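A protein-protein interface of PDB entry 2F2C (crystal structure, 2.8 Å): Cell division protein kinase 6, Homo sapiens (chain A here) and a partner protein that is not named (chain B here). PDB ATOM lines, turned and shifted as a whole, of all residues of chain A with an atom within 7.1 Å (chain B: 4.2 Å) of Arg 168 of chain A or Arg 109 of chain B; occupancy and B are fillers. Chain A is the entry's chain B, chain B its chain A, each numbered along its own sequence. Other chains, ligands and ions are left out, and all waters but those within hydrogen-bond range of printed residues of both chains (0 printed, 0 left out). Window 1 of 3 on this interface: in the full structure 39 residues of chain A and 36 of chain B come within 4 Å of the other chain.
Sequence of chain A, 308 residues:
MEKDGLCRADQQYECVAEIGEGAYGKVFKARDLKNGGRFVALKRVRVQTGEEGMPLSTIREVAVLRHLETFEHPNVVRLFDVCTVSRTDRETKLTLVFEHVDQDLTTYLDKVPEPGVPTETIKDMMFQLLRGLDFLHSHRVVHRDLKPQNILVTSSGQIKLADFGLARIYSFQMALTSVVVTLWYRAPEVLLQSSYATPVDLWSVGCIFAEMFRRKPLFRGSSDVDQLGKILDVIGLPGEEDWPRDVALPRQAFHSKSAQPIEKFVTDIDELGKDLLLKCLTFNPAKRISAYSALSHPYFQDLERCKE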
ATOM      1  N   LEU A  56      28.353  23.603  13.957  1.00  0.00           N
ATOM      2  CA  LEU A  56      28.601  22.976  15.246  1.00  0.00           C
ATOM      3  C   LEU A  56      28.006  23.819  16.374  1.00  0.00           C
ATOM      4  O   LEU A  56      27.186  23.339  17.167  1.00  0.00           O
ATOM      5  CB  LEU A  56      30.107  22.843  15.447  1.00  0.00           C
ATOM      6  CG  LEU A  56      30.671  21.969  16.562  1.00  0.00           C
ATOM      7  CD1 LEU A  56      32.156  21.798  16.303  1.00  0.00           C
ATOM      8  CD2 LEU A  56      30.431  22.551  17.940  1.00  0.00           C
ATOM      9  N   ARG A  60      24.811  22.734  19.296  1.00  0.00           N
ATOM     10  CA  ARG A  60      25.090  22.694  20.730  1.00  0.00           C
ATOM     11  C   ARG A  60      24.181  23.640  21.500  1.00  0.00           C
ATOM     12  O   ARG A  60      23.581  23.269  22.498  1.00  0.00           O
ATOM     13  CB  ARG A  60      26.543  23.085  21.015  1.00  0.00           C
ATOM     14  CG  ARG A  60      27.606  22.249  20.342  1.00  0.00           C
ATOM     15  CD  ARG A  60      28.361  21.296  21.259  1.00  0.00           C
ATOM     16  NE  ARG A  60      29.703  21.032  20.726  1.00  0.00           N
ATOM     17  CZ  ARG A  60      30.834  21.324  21.363  1.00  0.00           C
ATOM     18  NH1 ARG A  60      30.795  21.849  22.581  1.00  0.00           N
ATOM     19  NH2 ARG A  60      32.005  21.083  20.797  1.00  0.00           N
ATOM     20  N   VAL A  64      20.991  22.413  24.225  1.00  0.00           N
ATOM     21  CA  VAL A  64      21.034  22.669  25.655  1.00  0.00           C
ATOM     22  C   VAL A  64      19.702  23.305  26.028  1.00  0.00           C
ATOM     23  O   VAL A  64      18.911  22.719  26.791  1.00  0.00           O
ATOM     24  CB  VAL A  64      22.264  23.531  26.028  1.00  0.00           C
ATOM     25  CG1 VAL A  64      22.151  24.096  27.434  1.00  0.00           C
ATOM     26  CG2 VAL A  64      23.551  22.688  25.878  1.00  0.00           C
ATOM     27  N   HIS A  67      16.871  20.978  25.738  1.00  0.00           N
ATOM     28  CA  HIS A  67      16.974  19.932  26.746  1.00  0.00           C
ATOM     29  C   HIS A  67      16.468  20.358  28.124  1.00  0.00           C
ATOM     30  O   HIS A  67      15.976  19.541  28.886  1.00  0.00           O
ATOM     31  CB  HIS A  67      18.425  19.442  26.850  1.00  0.00           C
ATOM     32  CG  HIS A  67      18.590  18.202  27.673  1.00  0.00           C
ATOM     33  ND1 HIS A  67      19.566  18.074  28.642  1.00  0.00           N
ATOM     34  CD2 HIS A  67      17.895  17.039  27.681  1.00  0.00           C
ATOM     35  CE1 HIS A  67      19.472  16.880  29.203  1.00  0.00           C
ATOM     36  NE2 HIS A  67      18.464  16.236  28.642  1.00  0.00           N
ATOM     37  N   HIS A 139      23.146  20.138  36.076  1.00  0.00           N
ATOM     38  CA  HIS A 139      22.694  19.340  34.936  1.00  0.00           C
ATOM     39  C   HIS A 139      23.885  19.039  34.027  1.00  0.00           C
ATOM     40  O   HIS A 139      23.738  18.588  32.883  1.00  0.00           O
ATOM     41  CB  HIS A 139      21.572  20.055  34.199  1.00  0.00           C
ATOM     42  CG  HIS A 139      20.303  20.128  34.997  1.00  0.00           C
ATOM     43  ND1 HIS A 139      19.132  19.524  34.593  1.00  0.00           N
ATOM     44  CD2 HIS A 139      20.038  20.698  36.198  1.00  0.00           C
ATOM     45  CE1 HIS A 139      18.197  19.723  35.502  1.00  0.00           C
ATOM     46  NE2 HIS A 139      18.723  20.432  36.488  1.00  0.00           N
ATOM     47  N   ARG A 140      25.074  19.277  34.577  1.00  0.00           N
ATOM     48  CA  ARG A 140      26.335  18.933  33.950  1.00  0.00           C
ATOM     49  C   ARG A 140      26.676  19.774  32.721  1.00  0.00           C
ATOM     50  O   ARG A 140      27.517  19.365  31.914  1.00  0.00           O
ATOM     51  CB  ARG A 140      26.345  17.455  33.599  1.00  0.00           C
ATOM     52  CG  ARG A 140      26.233  16.542  34.779  1.00  0.00           C
ATOM     53  CD  ARG A 140      25.615  15.206  34.420  1.00  0.00           C
ATOM     54  NE  ARG A 140      26.246  14.617  33.231  1.00  0.00           N
ATOM     55  CZ  ARG A 140      27.276  13.783  33.277  1.00  0.00           C
ATOM     56  NH1 ARG A 140      27.783  13.457  34.468  1.00  0.00           N
ATOM     57  NH2 ARG A 140      27.785  13.285  32.153  1.00  0.00           N
ATOM     58  N   VAL A 141      26.019  20.928  32.585  1.00  0.00           N
ATOM     59  CA  VAL A 141      26.294  21.878  31.504  1.00  0.00           C
ATOM     60  C   VAL A 141      27.238  22.986  31.973  1.00  0.00           C
ATOM     61  O   VAL A 141      27.020  23.614  33.027  1.00  0.00           O
ATOM     62  CB  VAL A 141      24.994  22.555  30.986  1.00  0.00           C
ATOM     63  CG1 VAL A 141      25.290  23.698  30.005  1.00  0.00           C
ATOM     64  CG2 VAL A 141      24.072  21.539  30.369  1.00  0.00           C
ATOM     65  N   VAL A 142      28.278  23.247  31.188  1.00  0.00           N
ATOM     66  CA  VAL A 142      29.147  24.368  31.513  1.00  0.00           C
ATOM     67  C   VAL A 142      28.988  25.438  30.445  1.00  0.00           C
ATOM     68  O   VAL A 142      29.266  25.182  29.289  1.00  0.00           O
ATOM     69  CB  VAL A 142      30.609  23.920  31.644  1.00  0.00           C
ATOM     70  CG1 VAL A 142      31.433  24.979  32.339  1.00  0.00           C
ATOM     71  CG2 VAL A 142      30.681  22.638  32.445  1.00  0.00           C
ATOM     72  N   HIS A 143      28.496  26.617  30.824  1.00  0.00           N
ATOM     73  CA  HIS A 143      28.415  27.744  29.904  1.00  0.00           C
ATOM     74  C   HIS A 143      29.817  28.256  29.905  1.00  0.00           C
ATOM     75  O   HIS A 143      30.247  28.795  30.930  1.00  0.00           O
ATOM     76  CB  HIS A 143      27.501  28.851  30.459  1.00  0.00           C
ATOM     77  CG  HIS A 143      27.237  29.971  29.491  1.00  0.00           C
ATOM     78  ND1 HIS A 143      28.236  30.772  28.976  1.00  0.00           N
ATOM     79  CD2 HIS A 143      26.082  30.422  28.945  1.00  0.00           C
ATOM     80  CE1 HIS A 143      27.712  31.654  28.145  1.00  0.00           C
ATOM     81  NE2 HIS A 143      26.405  31.467  28.114  1.00  0.00           N
ATOM     82  N   ARG A 144      30.545  28.119  28.804  1.00  0.00           N
ATOM     83  CA  ARG A 144      31.950  28.505  28.842  1.00  0.00           C
ATOM     84  C   ARG A 144      32.201  29.804  28.108  1.00  0.00           C
ATOM     85  O   ARG A 144      33.138  29.910  27.312  1.00  0.00           O
ATOM     86  CB  ARG A 144      32.818  27.378  28.286  1.00  0.00           C
ATOM     87  CG  ARG A 144      32.599  26.081  29.034  1.00  0.00           C
ATOM     88  CD  ARG A 144      33.348  24.904  28.483  1.00  0.00           C
ATOM     89  NE  ARG A 144      33.017  24.725  27.081  1.00  0.00           N
ATOM     90  CZ  ARG A 144      33.607  23.857  26.273  1.00  0.00           C
ATOM     91  NH1 ARG A 144      34.574  23.059  26.733  1.00  0.00           N
ATOM     92  NH2 ARG A 144      33.229  23.792  25.002  1.00  0.00           N
ATOM     93  N   PHE A 164      24.560  30.197  23.946  1.00  0.00           N
ATOM     94  CA  PHE A 164      25.002  28.906  24.486  1.00  0.00           C
ATOM     95  C   PHE A 164      25.855  28.086  23.479  1.00  0.00           C
ATOM     96  O   PHE A 164      26.051  26.871  23.640  1.00  0.00           O
ATOM     97  CB  PHE A 164      23.781  28.116  25.004  1.00  0.00           C
ATOM     98  CG  PHE A 164      23.380  28.474  26.401  1.00  0.00           C
ATOM     99  CD1 PHE A 164      23.654  27.618  27.452  1.00  0.00           C
ATOM    100  CD2 PHE A 164      22.751  29.692  26.675  1.00  0.00           C
ATOM    101  CE1 PHE A 164      23.297  27.954  28.757  1.00  0.00           C
ATOM    102  CE2 PHE A 164      22.403  30.052  27.982  1.00  0.00           C
ATOM    103  CZ  PHE A 164      22.679  29.187  29.023  1.00  0.00           C
ATOM    104  N   GLY A 165      26.386  28.767  22.466  1.00  0.00           N
ATOM    105  CA  GLY A 165      27.069  28.103  21.345  1.00  0.00           C
ATOM    106  C   GLY A 165      28.434  27.484  21.620  1.00  0.00           C
ATOM    107  O   GLY A 165      29.069  26.936  20.706  1.00  0.00           O
ATOM    108  N   LEU A 166      28.872  27.583  22.875  1.00  0.00           N
ATOM    109  CA  LEU A 166      30.149  27.054  23.322  1.00  0.00           C
ATOM    110  C   LEU A 166      29.931  26.126  24.517  1.00  0.00           C
ATOM    111  O   LEU A 166      30.890  25.601  25.095  1.00  0.00           O
ATOM    112  CB  LEU A 166      31.055  28.215  23.728  1.00  0.00           C
ATOM    113  CG  LEU A 166      32.446  28.330  23.092  1.00  0.00           C
ATOM    114  CD1 LEU A 166      32.402  28.273  21.549  1.00  0.00           C
ATOM    115  CD2 LEU A 166      33.124  29.600  23.576  1.00  0.00           C
ATOM    116  N   ALA A 167      28.662  25.959  24.900  1.00  0.00           N
ATOM    117  CA  ALA A 167      28.288  25.140  26.041  1.00  0.00           C
ATOM    118  C   ALA A 167      28.210  23.673  25.626  1.00  0.00           C
ATOM    119  O   ALA A 167      28.014  23.348  24.440  1.00  0.00           O
ATOM    120  CB  ALA A 167      26.970  25.593  26.611  1.00  0.00           C
ATOM    121  N   ARG A 168      28.368  22.797  26.614  1.00  0.00           N
ATOM    122  CA  ARG A 168      28.237  21.380  26.415  1.00  0.00           C
ATOM    123  C   ARG A 168      28.081  20.616  27.724  1.00  0.00           C
ATOM    124  O   ARG A 168      28.450  21.109  28.799  1.00  0.00           O
ATOM    125  CB  ARG A 168      29.426  20.842  25.623  1.00  0.00           C
ATOM    126  CG  ARG A 168      30.784  21.250  26.097  1.00  0.00           C
ATOM    127  CD  ARG A 168      31.882  20.851  25.103  1.00  0.00           C
ATOM    128  NE  ARG A 168      32.176  19.422  25.190  1.00  0.00           N
ATOM    129  CZ  ARG A 168      32.483  18.649  24.175  1.00  0.00           C
ATOM    130  NH1 ARG A 168      32.521  19.136  22.950  1.00  0.00           N
ATOM    131  NH2 ARG A 168      32.722  17.368  24.378  1.00  0.00           N
ATOM    132  N   ILE A 169      27.510  19.422  27.624  1.00  0.00           N
ATOM    133  CA  ILE A 169      27.457  18.514  28.739  1.00  0.00           C
ATOM    134  C   ILE A 169      28.864  17.970  29.006  1.00  0.00           C
ATOM    135  O   ILE A 169      29.445  17.295  28.143  1.00  0.00           O
ATOM    136  CB  ILE A 169      26.483  17.390  28.393  1.00  0.00           C
ATOM    137  CG1 ILE A 169      25.075  17.983  28.178  1.00  0.00           C
ATOM    138  CG2 ILE A 169      26.570  16.285  29.418  1.00  0.00           C
ATOM    139  CD1 ILE A 169      23.899  17.027  28.450  1.00  0.00           C
ATOM    140  N   TYR A 170      29.427  18.265  30.177  1.00  0.00           N
ATOM    141  CA  TYR A 170      30.731  17.687  30.546  1.00  0.00           C
ATOM    142  C   TYR A 170      30.679  16.235  31.031  1.00  0.00           C
ATOM    143  O   TYR A 170      29.864  15.886  31.894  1.00  0.00           O
ATOM    144  CB  TYR A 170      31.431  18.511  31.634  1.00  0.00           C
ATOM    145  CG  TYR A 170      32.496  19.485  31.126  1.00  0.00           C
ATOM    146  CD1 TYR A 170      32.215  20.358  30.060  1.00  0.00           C
ATOM    147  CD2 TYR A 170      33.760  19.570  31.734  1.00  0.00           C
ATOM    148  CE1 TYR A 170      33.147  21.253  29.605  1.00  0.00           C
ATOM    149  CE2 TYR A 170      34.693  20.472  31.279  1.00  0.00           C
ATOM    150  CZ  TYR A 170      34.378  21.316  30.209  1.00  0.00           C
ATOM    151  OH  TYR A 170      35.273  22.253  29.710  1.00  0.00           O
ATOM    152  N   SER A 171      31.599  15.417  30.532  1.00  0.00           N
ATOM    153  CA  SER A 171      31.775  14.069  31.042  1.00  0.00           C
ATOM    154  C   SER A 171      33.252  13.759  31.262  1.00  0.00           C
ATOM    155  O   SER A 171      34.081  14.094  30.423  1.00  0.00           O
ATOM    156  CB  SER A 171      31.143  13.031  30.087  1.00  0.00           C
ATOM    157  OG  SER A 171      30.102  13.602  29.302  1.00  0.00           O
ATOM    158  N   MET A 174      36.475  13.312  28.767  1.00  0.00           N
ATOM    159  CA  MET A 174      36.220  13.933  27.443  1.00  0.00           C
ATOM    160  C   MET A 174      37.290  14.946  27.020  1.00  0.00           C
ATOM    161  O   MET A 174      37.813  15.707  27.831  1.00  0.00           O
ATOM    162  CB  MET A 174      34.825  14.563  27.334  1.00  0.00           C
ATOM    163  CG  MET A 174      34.632  15.820  28.139  1.00  0.00           C
ATOM    164  SD  MET A 174      33.095  16.698  27.756  1.00  0.00           S
ATOM    165  CE  MET A 174      33.827  18.197  27.138  1.00  0.00           C
ATOM    166  N   ALA A 175      37.596  14.939  25.731  1.00  0.00           N
ATOM    167  CA  ALA A 175      38.534  15.877  25.131  1.00  0.00           C
ATOM    168  C   ALA A 175      38.055  17.346  25.223  1.00  0.00           C
ATOM    169  O   ALA A 175      36.879  17.612  25.468  1.00  0.00           O
ATOM    170  CB  ALA A 175      38.807  15.470  23.692  1.00  0.00           C
ATOM    171  N   LEU A 176      38.972  18.288  25.052  1.00  0.00           N
ATOM    172  CA  LEU A 176      38.641  19.702  25.142  1.00  0.00           C
ATOM    173  C   LEU A 176      39.461  20.478  24.127  1.00  0.00           C
ATOM    174  O   LEU A 176      40.603  20.117  23.859  1.00  0.00           O
ATOM    175  CB  LEU A 176      38.946  20.226  26.547  1.00  0.00           C
ATOM    176  CG  LEU A 176      38.221  19.610  27.758  1.00  0.00           C
ATOM    177  CD1 LEU A 176      38.931  19.979  29.055  1.00  0.00           C
ATOM    178  CD2 LEU A 176      36.749  20.017  27.822  1.00  0.00           C
ATOM    179  N   THR A 177      38.891  21.529  23.544  1.00  0.00           N
ATOM    180  CA  THR A 177      39.697  22.475  22.765  1.00  0.00           C
ATOM    181  C   THR A 177      40.365  23.303  23.818  1.00  0.00           C
ATOM    182  O   THR A 177      39.806  23.445  24.912  1.00  0.00           O
ATOM    183  CB  THR A 177      38.845  23.439  21.901  1.00  0.00           C
ATOM    184  OG1 THR A 177      37.578  23.674  22.539  1.00  0.00           O
ATOM    185  CG2 THR A 177      38.498  22.845  20.528  1.00  0.00           C
ATOM    186  N   TYR A 196      40.118  22.310  32.063  1.00  0.00           N
ATOM    187  CA  TYR A 196      39.175  23.246  32.628  1.00  0.00           C
ATOM    188  C   TYR A 196      37.782  22.628  32.674  1.00  0.00           C
ATOM    189  O   TYR A 196      37.460  21.727  31.884  1.00  0.00           O
ATOM    190  CB  TYR A 196      39.202  24.574  31.852  1.00  0.00           C
ATOM    191  CG  TYR A 196      38.876  24.450  30.388  1.00  0.00           C
ATOM    192  CD1 TYR A 196      39.859  24.080  29.463  1.00  0.00           C
ATOM    193  CD2 TYR A 196      37.583  24.711  29.922  1.00  0.00           C
ATOM    194  CE1 TYR A 196      39.555  23.954  28.109  1.00  0.00           C
ATOM    195  CE2 TYR A 196      37.265  24.585  28.567  1.00  0.00           C
ATOM    196  CZ  TYR A 196      38.251  24.200  27.667  1.00  0.00           C
ATOM    197  OH  TYR A 196      37.942  24.087  26.328  1.00  0.00           O
ATOM    198  N   ASP B  69      34.946  10.393  21.470  1.00  0.00           N
ATOM    199  CA  ASP B  69      34.594  10.357  22.876  1.00  0.00           C
ATOM    200  C   ASP B  69      33.526   9.345  23.130  1.00  0.00           C
ATOM    201  O   ASP B  69      32.625   9.179  22.328  1.00  0.00           O
ATOM    202  CB  ASP B  69      34.141  11.734  23.328  1.00  0.00           C
ATOM    203  CG  ASP B  69      35.304  12.599  23.772  1.00  0.00           C
ATOM    204  OD1 ASP B  69      35.450  13.748  23.273  1.00  0.00           O
ATOM    205  OD2 ASP B  69      36.148  12.203  24.612  1.00  0.00           O
ATOM    206  N   SER B  71      30.921   9.153  24.479  1.00  0.00           N
ATOM    207  CA  SER B  71      29.506   9.439  24.554  1.00  0.00           C
ATOM    208  C   SER B  71      28.818   9.758  23.198  1.00  0.00           C
ATOM    209  O   SER B  71      27.580   9.846  23.117  1.00  0.00           O
ATOM    210  CB  SER B  71      29.248  10.496  25.613  1.00  0.00           C
ATOM    211  OG  SER B  71      28.954  11.653  24.932  1.00  0.00           O
ATOM    212  N   VAL B  72      29.605   9.883  22.134  1.00  0.00           N
ATOM    213  CA  VAL B  72      29.055  10.048  20.779  1.00  0.00           C
ATOM    214  C   VAL B  72      28.137   8.902  20.332  1.00  0.00           C
ATOM    215  O   VAL B  72      27.065   9.119  19.739  1.00  0.00           O
ATOM    216  CB  VAL B  72      30.181  10.168  19.754  1.00  0.00           C
ATOM    217  CG1 VAL B  72      29.604  10.344  18.347  1.00  0.00           C
ATOM    218  CG2 VAL B  72      31.097  11.325  20.131  1.00  0.00           C
ATOM    219  N   GLY B 105      25.666  13.634  16.291  1.00  0.00           N
ATOM    220  CA  GLY B 105      26.211  13.187  17.581  1.00  0.00           C
ATOM    221  C   GLY B 105      27.629  13.666  17.810  1.00  0.00           C
ATOM    222  O   GLY B 105      27.921  14.322  18.818  1.00  0.00           O
ATOM    223  N   SER B 106      28.506  13.387  16.855  1.00  0.00           N
ATOM    224  CA  SER B 106      29.891  13.777  16.986  1.00  0.00           C
ATOM    225  C   SER B 106      29.995  15.295  17.102  1.00  0.00           C
ATOM    226  O   SER B 106      30.810  15.820  17.856  1.00  0.00           O
ATOM    227  CB  SER B 106      30.696  13.278  15.798  1.00  0.00           C
ATOM    228  OG  SER B 106      30.531  14.142  14.693  1.00  0.00           O
ATOM    229  N   LYS B 107      29.138  15.993  16.369  1.00  0.00           N
ATOM    230  CA  LYS B 107      29.091  17.430  16.434  1.00  0.00           C
ATOM    231  C   LYS B 107      28.712  17.933  17.817  1.00  0.00           C
ATOM    232  O   LYS B 107      29.021  19.071  18.161  1.00  0.00           O
ATOM    233  CB  LYS B 107      28.126  17.985  15.390  1.00  0.00           C
ATOM    234  CG  LYS B 107      28.748  18.201  14.024  1.00  0.00           C
ATOM    235  CD  LYS B 107      27.783  18.958  13.129  1.00  0.00           C
ATOM    236  CE  LYS B 107      28.225  18.964  11.694  1.00  0.00           C
ATOM    237  NZ  LYS B 107      27.202  19.658  10.887  1.00  0.00           N
ATOM    238  N   ILE B 108      28.050  17.109  18.621  1.00  0.00           N
ATOM    239  CA  ILE B 108      27.597  17.591  19.945  1.00  0.00           C
ATOM    240  C   ILE B 108      28.465  17.085  21.100  1.00  0.00           C
ATOM    241  O   ILE B 108      28.758  17.858  22.005  1.00  0.00           O
ATOM    242  CB  ILE B 108      26.095  17.247  20.211  1.00  0.00           C
ATOM    243  CG1 ILE B 108      25.205  17.933  19.182  1.00  0.00           C
ATOM    244  CG2 ILE B 108      25.685  17.634  21.640  1.00  0.00           C
ATOM    245  CD1 ILE B 108      23.794  17.388  19.160  1.00  0.00           C
ATOM    246  N   ARG B 109      28.860  15.806  21.075  1.00  0.00           N
ATOM    247  CA  ARG B 109      29.529  15.216  22.228  1.00  0.00           C
ATOM    248  C   ARG B 109      31.035  14.996  22.073  1.00  0.00           C
ATOM    249  O   ARG B 109      31.633  14.250  22.848  1.00  0.00           O
ATOM    250  CB  ARG B 109      28.854  13.900  22.620  1.00  0.00           C
ATOM    251  CG  ARG B 109      27.511  14.042  23.368  1.00  0.00           C
ATOM    252  CD  ARG B 109      27.614  14.537  24.820  1.00  0.00           C
ATOM    253  NE  ARG B 109      26.303  14.485  25.461  1.00  0.00           N
ATOM    254  CZ  ARG B 109      26.004  13.754  26.538  1.00  0.00           C
ATOM    255  NH1 ARG B 109      26.921  13.014  27.121  1.00  0.00           N
ATOM    256  NH2 ARG B 109      24.781  13.763  27.043  1.00  0.00           N
ATOM    257  N   THR B 110      31.653  15.647  21.094  1.00  0.00           N
ATOM    258  CA  THR B 110      33.075  15.426  20.815  1.00  0.00           C
ATOM    259  C   THR B 110      33.769  16.681  20.258  1.00  0.00           C
ATOM    260  O   THR B 110      33.136  17.563  19.673  1.00  0.00           O
ATOM    261  CB  THR B 110      33.256  14.185  19.885  1.00  0.00           C
ATOM    262  OG1 THR B 110      34.346  13.369  20.344  1.00  0.00           O
ATOM    263  CG2 THR B 110      33.653  14.593  18.467  1.00  0.00           C
ATOM    264  N   GLU B 148      19.891  16.390  22.198  1.00  0.00           N
ATOM    265  CA  GLU B 148      20.465  15.884  23.446  1.00  0.00           C
ATOM    266  C   GLU B 148      19.526  14.879  24.165  1.00  0.00           C
ATOM    267  O   GLU B 148      18.341  14.745  23.794  1.00  0.00           O
ATOM    268  CB  GLU B 148      20.790  17.089  24.336  1.00  0.00           C
ATOM    269  CG  GLU B 148      21.909  16.903  25.337  1.00  0.00           C
ATOM    270  CD  GLU B 148      23.166  16.267  24.741  1.00  0.00           C
ATOM    271  OE1 GLU B 148      23.265  15.000  24.712  1.00  0.00           O
ATOM    272  OE2 GLU B 148      24.070  17.044  24.336  1.00  0.00           O
ATOM    273  N   ALA B 149      20.062  14.173  25.169  1.00  0.00           N
ATOM    274  CA  ALA B 149      19.341  13.118  25.926  1.00  0.00           C
ATOM    275  C   ALA B 149      20.174  12.551  27.071  1.00  0.00           C
ATOM    276  O   ALA B 149      21.394  12.596  27.037  1.00  0.00           O
ATOM    277  CB  ALA B 149      18.917  11.971  25.007  1.00  0.00           C
ATOM    278  N   LEU B 151      22.204   9.835  28.489  1.00  0.00           N
ATOM    279  CA  LEU B 151      22.865   8.668  27.909  1.00  0.00           C
ATOM    280  C   LEU B 151      23.260   7.704  28.996  1.00  0.00           C
ATOM    281  O   LEU B 151      23.765   8.133  30.042  1.00  0.00           O
ATOM    282  CB  LEU B 151      24.142   9.085  27.192  1.00  0.00           C
ATOM    283  CG  LEU B 151      23.946  10.136  26.129  1.00  0.00           C
ATOM    284  CD1 LEU B 151      25.279  10.443  25.470  1.00  0.00           C
ATOM    285  CD2 LEU B 151      22.953   9.574  25.139  1.00  0.00           C
ATOM    286  N   ASP B 154      26.200   8.712  30.834  1.00  0.00           N
ATOM    287  CA  ASP B 154      26.294   9.873  31.720  1.00  0.00           C
ATOM    288  C   ASP B 154      26.204   9.451  33.188  1.00  0.00           C
ATOM    289  O   ASP B 154      26.567  10.226  34.089  1.00  0.00           O
ATOM    290  CB  ASP B 154      25.156  10.872  31.480  1.00  0.00           C
ATOM    291  CG  ASP B 154      25.140  11.480  30.070  1.00  0.00           C
ATOM    292  OD1 ASP B 154      26.165  12.055  29.606  1.00  0.00           O
ATOM    293  OD2 ASP B 154      24.077  11.484  29.382  1.00  0.00           O
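Of chain B, only Arg 109 (3.6 Å) and Thr 110 (3.7 Å) come within 4 Å of Arg 168 of chain A.
Of chain A, only Arg 168, Ile 169 and Ser 171 come within 4 Å of Arg 109 of chain B.
Of the printed residues of chain B, Met 174 of chain A touches Asp 69 (3.3 Å).
Printed residues of chain B within 4 Å of Ser 171 of chain A: Arg 109 (3.9 Å).
Of the printed residues of chain B, Leu 56 of chain A touches Lys 107 (3.7 Å).
Tyr 196 of chain A touches none of the printed residues of chain B.
Arg 144 of chain A touches none of the printed residues of chain B.
Lys 107 of chain B touches Leu 56 of chain A.
Arg 60 of chain A touches Ile 108 of chain B (CD to O, 3.5 Å).
Arg 60 of chain A touches Thr 110 of chain B (NH2 to O, 3.9 Å).
Arg 109 of chain B touches Arg 168 of chain A (O to NH2, 3.6 Å).
Thr 110 of chain B touches Arg 168 of chain A (O to NH1, 3.7 Å).
Arg 109 of chain B touches Ile 169 of chain A.
Ile 169 of chain A touches Glu 148 of chain B (CD1 to CG, 3.7 Å).
OG of Ser 171 of chain A touches NH1 of Arg 109 of chain B, 3.9 Å away.
Met 174 of chain A touches Asp 69 of chain B.
OD2 of Asp 69 of chain B lies within hydrogen-bond range of N of Ala 175 of chain A, 3.3 Å away.
The guanidinium group of Arg 60 of chain A is in hydrogen-bond range of the backbone carbonyl oxygen of Lys 107 of chain B (3.3 Å).
The guanidinium group of Arg 140 of chain A lies within salt-bridge range of the side-chain carboxylate of Asp 154 of chain B (3.3 Å).
Hydrophobic or aromatic side chains of chain A within 4 Å of the printed part of chain B: Leu 56, Ile 169, Met 174 and Ala 175.
The side-chain carboxylate (OD1) of Asp 69 of chain B lies within hydrogen-bond range of the side-chain hydroxyl (OG1) of Thr 110 of chain B.
The guanidinium group (NH2) of Arg 109 of chain B is in salt-bridge range of the side-chain carboxylate (OE1) of Glu 148 of chain B.
NH1 of Arg 109 of chain B lies within salt-bridge range of OD1 of Asp 154 of chain B (2.8 Å).
The side-chain carboxylate (OD2) of Asp 154 of chain B lies within hydrogen-bond range of the backbone NH (N) of Leu 151 of chain B (2.7 Å).
The backbone NH (N) of Tyr 170 of chain A is in hydrogen-bond range of the backbone carbonyl oxygen (O) of Arg 140 of chain A.
The backbone NH (N) of Ser 171 of chain A sits at hydrogen-bond distance from the side-chain sulfur (SD) of Met 174 of chain A (3.4 Å).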
